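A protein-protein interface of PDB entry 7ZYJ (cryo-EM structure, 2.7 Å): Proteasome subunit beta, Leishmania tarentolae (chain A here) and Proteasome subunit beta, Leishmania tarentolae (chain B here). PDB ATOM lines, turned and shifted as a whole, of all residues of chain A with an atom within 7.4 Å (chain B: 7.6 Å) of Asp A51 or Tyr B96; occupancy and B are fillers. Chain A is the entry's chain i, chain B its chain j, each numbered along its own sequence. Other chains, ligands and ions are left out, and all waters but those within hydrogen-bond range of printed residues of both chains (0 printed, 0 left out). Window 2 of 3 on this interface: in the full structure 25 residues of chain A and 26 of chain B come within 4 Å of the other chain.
OD1 of Asp A51 sits at hydrogen-bond distance from OH of Tyr B96, 2.6 Å away.
OD2 of Asp A51 lies within salt-bridge range of NH2 of Arg B99 (2.7 Å).
Of the 18 printed residues of chain B, 4 touch a printed residue of chain A.
Along chain B the printed residues that touch a printed residue of chain A span positions 96 to 129.
Of the 21 printed residues of chain A, 4 touch a printed residue of chain B.
Printed residues of chain A that touch a printed residue of chain B: Thr A48, Ala A50, Asp A51 and Ala A54.
Hydrophobic or aromatic side chains of chain A that line the printed part of chain B: Ala A50 and Ala A54.
Among the printed residues, Asp or Glu carboxylates within 4 Å of a Lys or Arg side-chain nitrogen of the other chain: Asp A51 with Arg B99 (2.7 Å).
N of Thr A48 sits at hydrogen-bond distance from O of Ser A95, at 3.1 Å.
The side-chain carboxylate (OD2) of Asp A51 is in hydrogen-bond range of the backbone NH (N) of Ser A95 (3.2 Å).
O of Thr A48 lies within hydrogen-bond range of OG1 of Thr A52, at 3.4 Å.
Asp A51 touches just these residues of chain B: Tyr B96 and Arg B99.
Ala A50 touches three residues of chain B.
Of the printed residues of chain A, Arg B99 touches Thr A48 (3.8 Å) and Asp A51 (2.7 Å).
Of the printed residues of chain B, Ala A54 touches Tyr B96.
Printed residues of chain B within 4 Å of Thr A48: Arg B99 and Ile B127.
Printed residues of chain A within 4 Å of Ile B127: Thr A48 and Ala A50.
The nearest residue of chain B that does not touch Asp A51 is Ile B127 (5.4 Å).
The nearest residue of chain A that does not touch Tyr B96 is Val A94 (4.3 Å).
The nearest printed residue of chain A that does not touch Ile B127 is Asp A51 (5.4 Å).
Among the printed residues, pairs that only touch across the chains: Ala A54 with Tyr B96, Ala A50 with Tyr B96, Ala A50 with Ala B129, Ala A50 with Ile B127, Thr A48 with Ile B127 and Thr A48 with Arg B99.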
ATOM      1  N   ALA A  46      17.279 -16.693 -32.517  1.00  0.00           N
ATOM      2  CA  ALA A  46      17.110 -15.816 -33.665  1.00  0.00           C
ATOM      3  C   ALA A  46      15.716 -15.210 -33.623  1.00  0.00           C
ATOM      4  O   ALA A  46      14.788 -15.773 -33.037  1.00  0.00           O
ATOM      5  CB  ALA A  46      17.328 -16.563 -34.987  1.00  0.00           C
ATOM      6  N   GLY A  47      15.576 -14.052 -34.261  1.00  0.00           N
ATOM      7  CA  GLY A  47      14.318 -13.334 -34.238  1.00  0.00           C
ATOM      8  C   GLY A  47      14.351 -12.149 -33.297  1.00  0.00           C
ATOM      9  O   GLY A  47      15.390 -11.499 -33.152  1.00  0.00           O
ATOM     10  N   THR A  48      13.222 -11.854 -32.659  1.00  0.00           N
ATOM     11  CA  THR A  48      13.162 -10.755 -31.704  1.00  0.00           C
ATOM     12  C   THR A  48      14.102 -11.027 -30.537  1.00  0.00           C
ATOM     13  O   THR A  48      13.908 -11.985 -29.784  1.00  0.00           O
ATOM     14  CB  THR A  48      11.730 -10.569 -31.204  1.00  0.00           C
ATOM     15  OG1 THR A  48      10.835 -10.513 -32.320  1.00  0.00           O
ATOM     16  CG2 THR A  48      11.610  -9.281 -30.407  1.00  0.00           C
ATOM     17  N   SER A  49      15.126 -10.181 -30.396  1.00  0.00           N
ATOM     18  CA  SER A  49      16.148 -10.415 -29.381  1.00  0.00           C
ATOM     19  C   SER A  49      15.560 -10.378 -27.977  1.00  0.00           C
ATOM     20  O   SER A  49      15.968 -11.157 -27.108  1.00  0.00           O
ATOM     21  CB  SER A  49      17.269  -9.387 -29.519  1.00  0.00           C
ATOM     22  OG  SER A  49      18.015  -9.602 -30.704  1.00  0.00           O
ATOM     23  N   ALA A  50      14.609  -9.475 -27.733  1.00  0.00           N
ATOM     24  CA  ALA A  50      13.995  -9.388 -26.412  1.00  0.00           C
ATOM     25  C   ALA A  50      13.269 -10.679 -26.059  1.00  0.00           C
ATOM     26  O   ALA A  50      13.408 -11.199 -24.947  1.00  0.00           O
ATOM     27  CB  ALA A  50      13.039  -8.196 -26.357  1.00  0.00           C
ATOM     28  N   ASP A  51      12.492 -11.216 -27.003  1.00  0.00           N
ATOM     29  CA  ASP A  51      11.755 -12.449 -26.748  1.00  0.00           C
ATOM     30  C   ASP A  51      12.698 -13.620 -26.509  1.00  0.00           C
ATOM     31  O   ASP A  51      12.490 -14.414 -25.583  1.00  0.00           O
ATOM     32  CB  ASP A  51      10.822 -12.747 -27.920  1.00  0.00           C
ATOM     33  CG  ASP A  51       9.611 -11.841 -27.943  1.00  0.00           C
ATOM     34  OD1 ASP A  51       9.239 -11.319 -26.873  1.00  0.00           O
ATOM     35  OD2 ASP A  51       9.030 -11.651 -29.031  1.00  0.00           O
ATOM     36  N   THR A  52      13.738 -13.744 -27.337  1.00  0.00           N
ATOM     37  CA  THR A  52      14.705 -14.821 -27.160  1.00  0.00           C
ATOM     38  C   THR A  52      15.387 -14.728 -25.804  1.00  0.00           C
ATOM     39  O   THR A  52      15.472 -15.723 -25.074  1.00  0.00           O
ATOM     40  CB  THR A  52      15.741 -14.784 -28.284  1.00  0.00           C
ATOM     41  OG1 THR A  52      15.121 -15.152 -29.523  1.00  0.00           O
ATOM     42  CG2 THR A  52      16.880 -15.740 -27.989  1.00  0.00           C
ATOM     43  N   GLU A  53      15.868 -13.537 -25.446  1.00  0.00           N
ATOM     44  CA  GLU A  53      16.526 -13.345 -24.160  1.00  0.00           C
ATOM     45  C   GLU A  53      15.595 -13.678 -23.003  1.00  0.00           C
ATOM     46  O   GLU A  53      15.988 -14.392 -22.075  1.00  0.00           O
ATOM     47  CB  GLU A  53      17.026 -11.906 -24.041  1.00  0.00           C
ATOM     48  CG  GLU A  53      17.909 -11.646 -22.835  1.00  0.00           C
ATOM     49  CD  GLU A  53      19.332 -12.120 -23.041  1.00  0.00           C
ATOM     50  OE1 GLU A  53      19.767 -12.200 -24.208  1.00  0.00           O
ATOM     51  OE2 GLU A  53      20.014 -12.412 -22.036  1.00  0.00           O
ATOM     52  N   ALA A  54      14.351 -13.196 -23.057  1.00  0.00           N
ATOM     53  CA  ALA A  54      13.417 -13.430 -21.962  1.00  0.00           C
ATOM     54  C   ALA A  54      13.103 -14.911 -21.810  1.00  0.00           C
ATOM     55  O   ALA A  54      13.149 -15.452 -20.697  1.00  0.00           O
ATOM     56  CB  ALA A  54      12.138 -12.629 -22.189  1.00  0.00           C
ATOM     57  N   VAL A  55      12.785 -15.590 -22.916  1.00  0.00           N
ATOM     58  CA  VAL A  55      12.407 -16.995 -22.818  1.00  0.00           C
ATOM     59  C   VAL A  55      13.595 -17.842 -22.371  1.00  0.00           C
ATOM     60  O   VAL A  55      13.450 -18.731 -21.522  1.00  0.00           O
ATOM     61  CB  VAL A  55      11.792 -17.490 -24.144  1.00  0.00           C
ATOM     62  CG1 VAL A  55      12.838 -17.653 -25.239  1.00  0.00           C
ATOM     63  CG2 VAL A  55      11.039 -18.791 -23.925  1.00  0.00           C
ATOM     64  N   THR A  56      14.792 -17.565 -22.899  1.00  0.00           N
ATOM     65  CA  THR A  56      15.961 -18.340 -22.503  1.00  0.00           C
ATOM     66  C   THR A  56      16.291 -18.123 -21.033  1.00  0.00           C
ATOM     67  O   THR A  56      16.575 -19.081 -20.307  1.00  0.00           O
ATOM     68  CB  THR A  56      17.159 -17.988 -23.384  1.00  0.00           C
ATOM     69  OG1 THR A  56      17.310 -16.565 -23.449  1.00  0.00           O
ATOM     70  CG2 THR A  56      16.974 -18.547 -24.786  1.00  0.00           C
ATOM     71  N   ASN A  57      16.241 -16.870 -20.568  1.00  0.00           N
ATOM     72  CA  ASN A  57      16.528 -16.594 -19.166  1.00  0.00           C
ATOM     73  C   ASN A  57      15.515 -17.266 -18.252  1.00  0.00           C
ATOM     74  O   ASN A  57      15.887 -17.863 -17.234  1.00  0.00           O
ATOM     75  CB  ASN A  57      16.550 -15.086 -18.921  1.00  0.00           C
ATOM     76  CG  ASN A  57      17.844 -14.442 -19.365  1.00  0.00           C
ATOM     77  OD1 ASN A  57      18.887 -15.091 -19.416  1.00  0.00           O
ATOM     78  ND2 ASN A  57      17.783 -13.157 -19.691  1.00  0.00           N
ATOM     79  N   HIS A  86       6.045 -22.893 -23.628  1.00  0.00           N
ATOM     80  CA  HIS A  86       5.952 -21.441 -23.510  1.00  0.00           C
ATOM     81  C   HIS A  86       5.724 -20.783 -24.864  1.00  0.00           C
ATOM     82  O   HIS A  86       4.913 -19.858 -24.982  1.00  0.00           O
ATOM     83  CB  HIS A  86       7.204 -20.873 -22.848  1.00  0.00           C
ATOM     84  CG  HIS A  86       7.157 -19.388 -22.668  1.00  0.00           C
ATOM     85  ND1 HIS A  86       7.678 -18.510 -23.594  1.00  0.00           N
ATOM     86  CD2 HIS A  86       6.614 -18.625 -21.692  1.00  0.00           C
ATOM     87  CE1 HIS A  86       7.482 -17.270 -23.181  1.00  0.00           C
ATOM     88  NE2 HIS A  86       6.839 -17.313 -22.028  1.00  0.00           N
ATOM     89  N   LEU A  87       6.429 -21.242 -25.901  1.00  0.00           N
ATOM     90  CA  LEU A  87       6.279 -20.625 -27.215  1.00  0.00           C
ATOM     91  C   LEU A  87       4.913 -20.924 -27.819  1.00  0.00           C
ATOM     92  O   LEU A  87       4.335 -20.072 -28.504  1.00  0.00           O
ATOM     93  CB  LEU A  87       7.398 -21.086 -28.146  1.00  0.00           C
ATOM     94  CG  LEU A  87       8.763 -20.458 -27.861  1.00  0.00           C
ATOM     95  CD1 LEU A  87       9.770 -20.844 -28.926  1.00  0.00           C
ATOM     96  CD2 LEU A  87       8.647 -18.947 -27.757  1.00  0.00           C
ATOM     97  N   TYR A  90       1.802 -18.719 -26.552  1.00  0.00           N
ATOM     98  CA  TYR A  90       1.640 -17.365 -27.062  1.00  0.00           C
ATOM     99  C   TYR A  90       1.349 -17.324 -28.557  1.00  0.00           C
ATOM    100  O   TYR A  90       1.363 -16.241 -29.149  1.00  0.00           O
ATOM    101  CB  TYR A  90       2.880 -16.533 -26.737  1.00  0.00           C
ATOM    102  CG  TYR A  90       2.920 -16.081 -25.297  1.00  0.00           C
ATOM    103  CD1 TYR A  90       2.028 -15.127 -24.825  1.00  0.00           C
ATOM    104  CD2 TYR A  90       3.838 -16.617 -24.405  1.00  0.00           C
ATOM    105  CE1 TYR A  90       2.054 -14.715 -23.509  1.00  0.00           C
ATOM    106  CE2 TYR A  90       3.872 -16.210 -23.086  1.00  0.00           C
ATOM    107  CZ  TYR A  90       2.977 -15.259 -22.644  1.00  0.00           C
ATOM    108  OH  TYR A  90       3.005 -14.849 -21.331  1.00  0.00           O
ATOM    109  N   GLY A  92       2.920 -17.965 -31.204  1.00  0.00           N
ATOM    110  CA  GLY A  92       3.950 -17.430 -32.067  1.00  0.00           C
ATOM    111  C   GLY A  92       4.195 -15.943 -31.950  1.00  0.00           C
ATOM    112  O   GLY A  92       5.072 -15.423 -32.651  1.00  0.00           O
ATOM    113  N   HIS A  93       3.456 -15.237 -31.092  1.00  0.00           N
ATOM    114  CA  HIS A  93       3.686 -13.808 -30.925  1.00  0.00           C
ATOM    115  C   HIS A  93       4.977 -13.522 -30.174  1.00  0.00           C
ATOM    116  O   HIS A  93       5.536 -12.430 -30.320  1.00  0.00           O
ATOM    117  CB  HIS A  93       2.498 -13.167 -30.210  1.00  0.00           C
ATOM    118  CG  HIS A  93       1.223 -13.237 -30.989  1.00  0.00           C
ATOM    119  ND1 HIS A  93       0.033 -13.655 -30.434  1.00  0.00           N
ATOM    120  CD2 HIS A  93       0.953 -12.946 -32.283  1.00  0.00           C
ATOM    121  CE1 HIS A  93      -0.915 -13.618 -31.352  1.00  0.00           C
ATOM    122  NE2 HIS A  93      -0.384 -13.190 -32.482  1.00  0.00           N
ATOM    123  N   VAL A  94       5.461 -14.472 -29.378  1.00  0.00           N
ATOM    124  CA  VAL A  94       6.817 -14.417 -28.835  1.00  0.00           C
ATOM    125  C   VAL A  94       7.707 -15.003 -29.928  1.00  0.00           C
ATOM    126  O   VAL A  94       7.937 -16.210 -30.000  1.00  0.00           O
ATOM    127  CB  VAL A  94       6.938 -15.162 -27.508  1.00  0.00           C
ATOM    128  CG1 VAL A  94       8.390 -15.247 -27.065  1.00  0.00           C
ATOM    129  CG2 VAL A  94       6.096 -14.481 -26.442  1.00  0.00           C
ATOM    130  N   SER A  95       8.189 -14.132 -30.811  1.00  0.00           N
ATOM    131  CA  SER A  95       8.893 -14.555 -32.020  1.00  0.00           C
ATOM    132  C   SER A  95      10.342 -14.860 -31.668  1.00  0.00           C
ATOM    133  O   SER A  95      11.204 -13.981 -31.648  1.00  0.00           O
ATOM    134  CB  SER A  95       8.790 -13.486 -33.101  1.00  0.00           C
ATOM    135  OG  SER A  95       9.346 -12.260 -32.662  1.00  0.00           O
ATOM    136  N   ALA A  96      10.611 -16.133 -31.385  1.00  0.00           N
ATOM    137  CA  ALA A  96      11.956 -16.595 -31.057  1.00  0.00           C
ATOM    138  C   ALA A  96      12.148 -17.973 -31.672  1.00  0.00           C
ATOM    139  O   ALA A  96      11.448 -18.921 -31.301  1.00  0.00           O
ATOM    140  CB  ALA A  96      12.176 -16.635 -29.545  1.00  0.00           C
ATOM    141  N   LEU A  98      14.677 -21.006 -31.877  1.00  0.00           N
ATOM    142  CA  LEU A  98      15.748 -21.453 -31.003  1.00  0.00           C
ATOM    143  C   LEU A  98      16.394 -22.719 -31.543  1.00  0.00           C
ATOM    144  O   LEU A  98      15.725 -23.585 -32.110  1.00  0.00           O
ATOM    145  CB  LEU A  98      15.224 -21.701 -29.588  1.00  0.00           C
ATOM    146  CG  LEU A  98      14.429 -20.545 -28.981  1.00  0.00           C
ATOM    147  CD1 LEU A  98      13.614 -21.022 -27.797  1.00  0.00           C
ATOM    148  CD2 LEU A  98      15.356 -19.412 -28.578  1.00  0.00           C
ATOM    149  N   PHE B  63       7.552   6.633 -17.553  1.00  0.00           N
ATOM    150  CA  PHE B  63       8.611   5.665 -17.308  1.00  0.00           C
ATOM    151  C   PHE B  63       9.673   6.220 -16.371  1.00  0.00           C
ATOM    152  O   PHE B  63      10.212   5.477 -15.548  1.00  0.00           O
ATOM    153  CB  PHE B  63       9.239   5.228 -18.632  1.00  0.00           C
ATOM    154  CG  PHE B  63      10.082   3.993 -18.521  1.00  0.00           C
ATOM    155  CD1 PHE B  63       9.492   2.744 -18.423  1.00  0.00           C
ATOM    156  CD2 PHE B  63      11.463   4.079 -18.508  1.00  0.00           C
ATOM    157  CE1 PHE B  63      10.265   1.605 -18.317  1.00  0.00           C
ATOM    158  CE2 PHE B  63      12.239   2.944 -18.403  1.00  0.00           C
ATOM    159  CZ  PHE B  63      11.640   1.706 -18.307  1.00  0.00           C
ATOM    160  N   MET B  90      16.971  -4.122 -14.563  1.00  0.00           N
ATOM    161  CA  MET B  90      15.665  -3.737 -14.042  1.00  0.00           C
ATOM    162  C   MET B  90      14.848  -3.010 -15.102  1.00  0.00           C
ATOM    163  O   MET B  90      13.646  -3.254 -15.249  1.00  0.00           O
ATOM    164  CB  MET B  90      15.837  -2.875 -12.791  1.00  0.00           C
ATOM    165  CG  MET B  90      14.574  -2.166 -12.333  1.00  0.00           C
ATOM    166  SD  MET B  90      14.907  -0.906 -11.088  1.00  0.00           S
ATOM    167  CE  MET B  90      14.831   0.581 -12.079  1.00  0.00           C
ATOM    168  N   ILE B  91      15.488  -2.115 -15.862  1.00  0.00           N
ATOM    169  CA  ILE B  91      14.777  -1.454 -16.955  1.00  0.00           C
ATOM    170  C   ILE B  91      14.344  -2.462 -18.011  1.00  0.00           C
ATOM    171  O   ILE B  91      13.241  -2.358 -18.561  1.00  0.00           O
ATOM    172  CB  ILE B  91      15.633  -0.339 -17.583  1.00  0.00           C
ATOM    173  CG1 ILE B  91      15.884   0.781 -16.582  1.00  0.00           C
ATOM    174  CG2 ILE B  91      14.967   0.219 -18.833  1.00  0.00           C
ATOM    175  CD1 ILE B  91      16.887   1.765 -17.080  1.00  0.00           C
ATOM    176  N   THR B  92      15.198  -3.439 -18.321  1.00  0.00           N
ATOM    177  CA  THR B  92      14.828  -4.466 -19.289  1.00  0.00           C
ATOM    178  C   THR B  92      13.595  -5.230 -18.826  1.00  0.00           C
ATOM    179  O   THR B  92      12.665  -5.467 -19.606  1.00  0.00           O
ATOM    180  CB  THR B  92      16.002  -5.422 -19.510  1.00  0.00           C
ATOM    181  OG1 THR B  92      17.107  -4.705 -20.076  1.00  0.00           O
ATOM    182  CG2 THR B  92      15.604  -6.554 -20.441  1.00  0.00           C
ATOM    183  N   SER B  93      13.566  -5.611 -17.549  1.00  0.00           N
ATOM    184  CA  SER B  93      12.414  -6.336 -17.023  1.00  0.00           C
ATOM    185  C   SER B  93      11.158  -5.472 -17.037  1.00  0.00           C
ATOM    186  O   SER B  93      10.077  -5.946 -17.404  1.00  0.00           O
ATOM    187  CB  SER B  93      12.708  -6.839 -15.611  1.00  0.00           C
ATOM    188  OG  SER B  93      12.809  -5.764 -14.696  1.00  0.00           O
ATOM    189  N   MET B  94      11.282  -4.198 -16.648  1.00  0.00           N
ATOM    190  CA  MET B  94      10.125  -3.306 -16.659  1.00  0.00           C
ATOM    191  C   MET B  94       9.578  -3.127 -18.068  1.00  0.00           C
ATOM    192  O   MET B  94       8.359  -3.122 -18.273  1.00  0.00           O
ATOM    193  CB  MET B  94      10.493  -1.949 -16.057  1.00  0.00           C
ATOM    194  CG  MET B  94      10.887  -1.991 -14.595  1.00  0.00           C
ATOM    195  SD  MET B  94      11.467  -0.395 -13.989  1.00  0.00           S
ATOM    196  CE  MET B  94      10.026   0.623 -14.285  1.00  0.00           C
ATOM    197  N   LEU B  95      10.465  -2.973 -19.052  1.00  0.00           N
ATOM    198  CA  LEU B  95      10.020  -2.817 -20.431  1.00  0.00           C
ATOM    199  C   LEU B  95       9.410  -4.100 -20.977  1.00  0.00           C
ATOM    200  O   LEU B  95       8.471  -4.041 -21.778  1.00  0.00           O
ATOM    201  CB  LEU B  95      11.187  -2.366 -21.309  1.00  0.00           C
ATOM    202  CG  LEU B  95      11.614  -0.906 -21.154  1.00  0.00           C
ATOM    203  CD1 LEU B  95      12.911  -0.646 -21.896  1.00  0.00           C
ATOM    204  CD2 LEU B  95      10.519   0.027 -21.640  1.00  0.00           C
ATOM    205  N   TYR B  96       9.922  -5.262 -20.565  1.00  0.00           N
ATOM    206  CA  TYR B  96       9.373  -6.509 -21.084  1.00  0.00           C
ATOM    207  C   TYR B  96       8.070  -6.904 -20.401  1.00  0.00           C
ATOM    208  O   TYR B  96       7.300  -7.685 -20.968  1.00  0.00           O
ATOM    209  CB  TYR B  96      10.389  -7.644 -20.958  1.00  0.00           C
ATOM    210  CG  TYR B  96      10.065  -8.810 -21.864  1.00  0.00           C
ATOM    211  CD1 TYR B  96      10.438  -8.797 -23.201  1.00  0.00           C
ATOM    212  CD2 TYR B  96       9.365  -9.911 -21.391  1.00  0.00           C
ATOM    213  CE1 TYR B  96      10.135  -9.853 -24.037  1.00  0.00           C
ATOM    214  CE2 TYR B  96       9.054 -10.970 -22.220  1.00  0.00           C
ATOM    215  CZ  TYR B  96       9.443 -10.936 -23.541  1.00  0.00           C
ATOM    216  OH  TYR B  96       9.140 -11.990 -24.369  1.00  0.00           O
ATOM    217  N   GLU B  97       7.800  -6.393 -19.195  1.00  0.00           N
ATOM    218  CA  GLU B  97       6.501  -6.665 -18.582  1.00  0.00           C
ATOM    219  C   GLU B  97       5.360  -6.163 -19.455  1.00  0.00           C
ATOM    220  O   GLU B  97       4.335  -6.840 -19.586  1.00  0.00           O
ATOM    221  CB  GLU B  97       6.405  -6.040 -17.190  1.00  0.00           C
ATOM    222  CG  GLU B  97       7.386  -6.587 -16.173  1.00  0.00           C
ATOM    223  CD  GLU B  97       7.613  -5.635 -15.014  1.00  0.00           C
ATOM    224  OE1 GLU B  97       7.059  -4.516 -15.045  1.00  0.00           O
ATOM    225  OE2 GLU B  97       8.346  -6.005 -14.073  1.00  0.00           O
ATOM    226  N   ALA B  98       5.513  -4.984 -20.048  1.00  0.00           N
ATOM    227  CA  ALA B  98       4.538  -4.466 -21.004  1.00  0.00           C
ATOM    228  C   ALA B  98       4.973  -4.823 -22.425  1.00  0.00           C
ATOM    229  O   ALA B  98       5.131  -3.972 -23.293  1.00  0.00           O
ATOM    230  CB  ALA B  98       4.372  -2.960 -20.827  1.00  0.00           C
ATOM    231  N   ARG B  99       5.173  -6.120 -22.652  1.00  0.00           N
ATOM    232  CA  ARG B  99       5.665  -6.565 -23.950  1.00  0.00           C
ATOM    233  C   ARG B  99       4.648  -6.363 -25.064  1.00  0.00           C
ATOM    234  O   ARG B  99       5.036  -6.058 -26.198  1.00  0.00           O
ATOM    235  CB  ARG B  99       6.075  -8.038 -23.893  1.00  0.00           C
ATOM    236  CG  ARG B  99       6.981  -8.463 -25.036  1.00  0.00           C
ATOM    237  CD  ARG B  99       6.235  -9.279 -26.071  1.00  0.00           C
ATOM    238  NE  ARG B  99       7.066  -9.573 -27.233  1.00  0.00           N
ATOM    239  CZ  ARG B  99       7.127  -8.816 -28.320  1.00  0.00           C
ATOM    240  NH1 ARG B  99       6.412  -7.710 -28.433  1.00  0.00           N
ATOM    241  NH2 ARG B  99       7.922  -9.183 -29.321  1.00  0.00           N
ATOM    242  N   PHE B 100       3.358  -6.518 -24.771  1.00  0.00           N
ATOM    243  CA  PHE B 100       2.305  -6.313 -25.755  1.00  0.00           C
ATOM    244  C   PHE B 100       1.570  -4.994 -25.568  1.00  0.00           C
ATOM    245  O   PHE B 100       0.717  -4.651 -26.393  1.00  0.00           O
ATOM    246  CB  PHE B 100       1.314  -7.480 -25.709  1.00  0.00           C
ATOM    247  CG  PHE B 100       1.957  -8.820 -25.927  1.00  0.00           C
ATOM    248  CD1 PHE B 100       2.508  -9.144 -27.155  1.00  0.00           C
ATOM    249  CD2 PHE B 100       2.020  -9.748 -24.903  1.00  0.00           C
ATOM    250  CE1 PHE B 100       3.105 -10.372 -27.359  1.00  0.00           C
ATOM    251  CE2 PHE B 100       2.616 -10.979 -25.101  1.00  0.00           C
ATOM    252  CZ  PHE B 100       3.159 -11.291 -26.330  1.00  0.00           C
ATOM    253  N   GLY B 101       1.874  -4.253 -24.505  1.00  0.00           N
ATOM    254  CA  GLY B 101       1.360  -2.918 -24.298  1.00  0.00           C
ATOM    255  C   GLY B 101       2.476  -1.892 -24.216  1.00  0.00           C
ATOM    256  O   GLY B 101       2.489  -1.036 -23.326  1.00  0.00           O
ATOM    257  N   TRP B 103       5.658   0.472 -23.665  1.00  0.00           N
ATOM    258  CA  TRP B 103       6.014   1.873 -23.526  1.00  0.00           C
ATOM    259  C   TRP B 103       6.749   2.335 -24.776  1.00  0.00           C
ATOM    260  O   TRP B 103       7.430   1.556 -25.446  1.00  0.00           O
ATOM    261  CB  TRP B 103       6.895   2.091 -22.296  1.00  0.00           C
ATOM    262  CG  TRP B 103       6.276   1.646 -21.012  1.00  0.00           C
ATOM    263  CD1 TRP B 103       6.587   0.528 -20.297  1.00  0.00           C
ATOM    264  CD2 TRP B 103       5.242   2.315 -20.281  1.00  0.00           C
ATOM    265  NE1 TRP B 103       5.809   0.455 -19.169  1.00  0.00           N
ATOM    266  CE2 TRP B 103       4.975   1.541 -19.136  1.00  0.00           C
ATOM    267  CE3 TRP B 103       4.516   3.491 -20.486  1.00  0.00           C
ATOM    268  CZ2 TRP B 103       4.011   1.905 -18.199  1.00  0.00           C
ATOM    269  CZ3 TRP B 103       3.561   3.850 -19.555  1.00  0.00           C
ATOM    270  CH2 TRP B 103       3.317   3.060 -18.426  1.00  0.00           C
ATOM    271  N   LEU B 126      12.174  -0.588 -27.347  1.00  0.00           N
ATOM    272  CA  LEU B 126      10.979  -0.250 -26.587  1.00  0.00           C
ATOM    273  C   LEU B 126      10.455  -1.426 -25.774  1.00  0.00           C
ATOM    274  O   LEU B 126       9.660  -1.217 -24.851  1.00  0.00           O
ATOM    275  CB  LEU B 126       9.881   0.268 -27.521  1.00  0.00           C
ATOM    276  CG  LEU B 126       9.066  -0.740 -28.335  1.00  0.00           C
ATOM    277  CD1 LEU B 126       7.821  -0.069 -28.889  1.00  0.00           C
ATOM    278  CD2 LEU B 126       9.887  -1.341 -29.464  1.00  0.00           C
ATOM    279  N   ILE B 127      10.880  -2.649 -26.088  1.00  0.00           N
ATOM    280  CA  ILE B 127      10.482  -3.834 -25.341  1.00  0.00           C
ATOM    281  C   ILE B 127      11.625  -4.378 -24.493  1.00  0.00           C
ATOM    282  O   ILE B 127      11.488  -5.449 -23.893  1.00  0.00           O
ATOM    283  CB  ILE B 127       9.924  -4.924 -26.271  1.00  0.00           C
ATOM    284  CG1 ILE B 127      10.919  -5.235 -27.390  1.00  0.00           C
ATOM    285  CG2 ILE B 127       8.583  -4.497 -26.841  1.00  0.00           C
ATOM    286  CD1 ILE B 127      10.425  -6.273 -28.370  1.00  0.00           C
ATOM    287  N   GLY B 128      12.752  -3.673 -24.433  1.00  0.00           N
ATOM    288  CA  GLY B 128      13.818  -4.001 -23.506  1.00  0.00           C
ATOM    289  C   GLY B 128      14.981  -4.782 -24.075  1.00  0.00           C
ATOM    290  O   GLY B 128      15.865  -5.173 -23.305  1.00  0.00           O
ATOM    291  N   ALA B 129      15.022  -5.030 -25.384  1.00  0.00           N
ATOM    292  CA  ALA B 129      16.116  -5.793 -25.974  1.00  0.00           C
ATOM    293  C   ALA B 129      17.437  -5.062 -25.769  1.00  0.00           C
ATOM    294  O   ALA B 129      17.676  -4.023 -26.395  1.00  0.00           O
ATOM    295  CB  ALA B 129      15.865  -6.036 -27.463  1.00  0.00           C
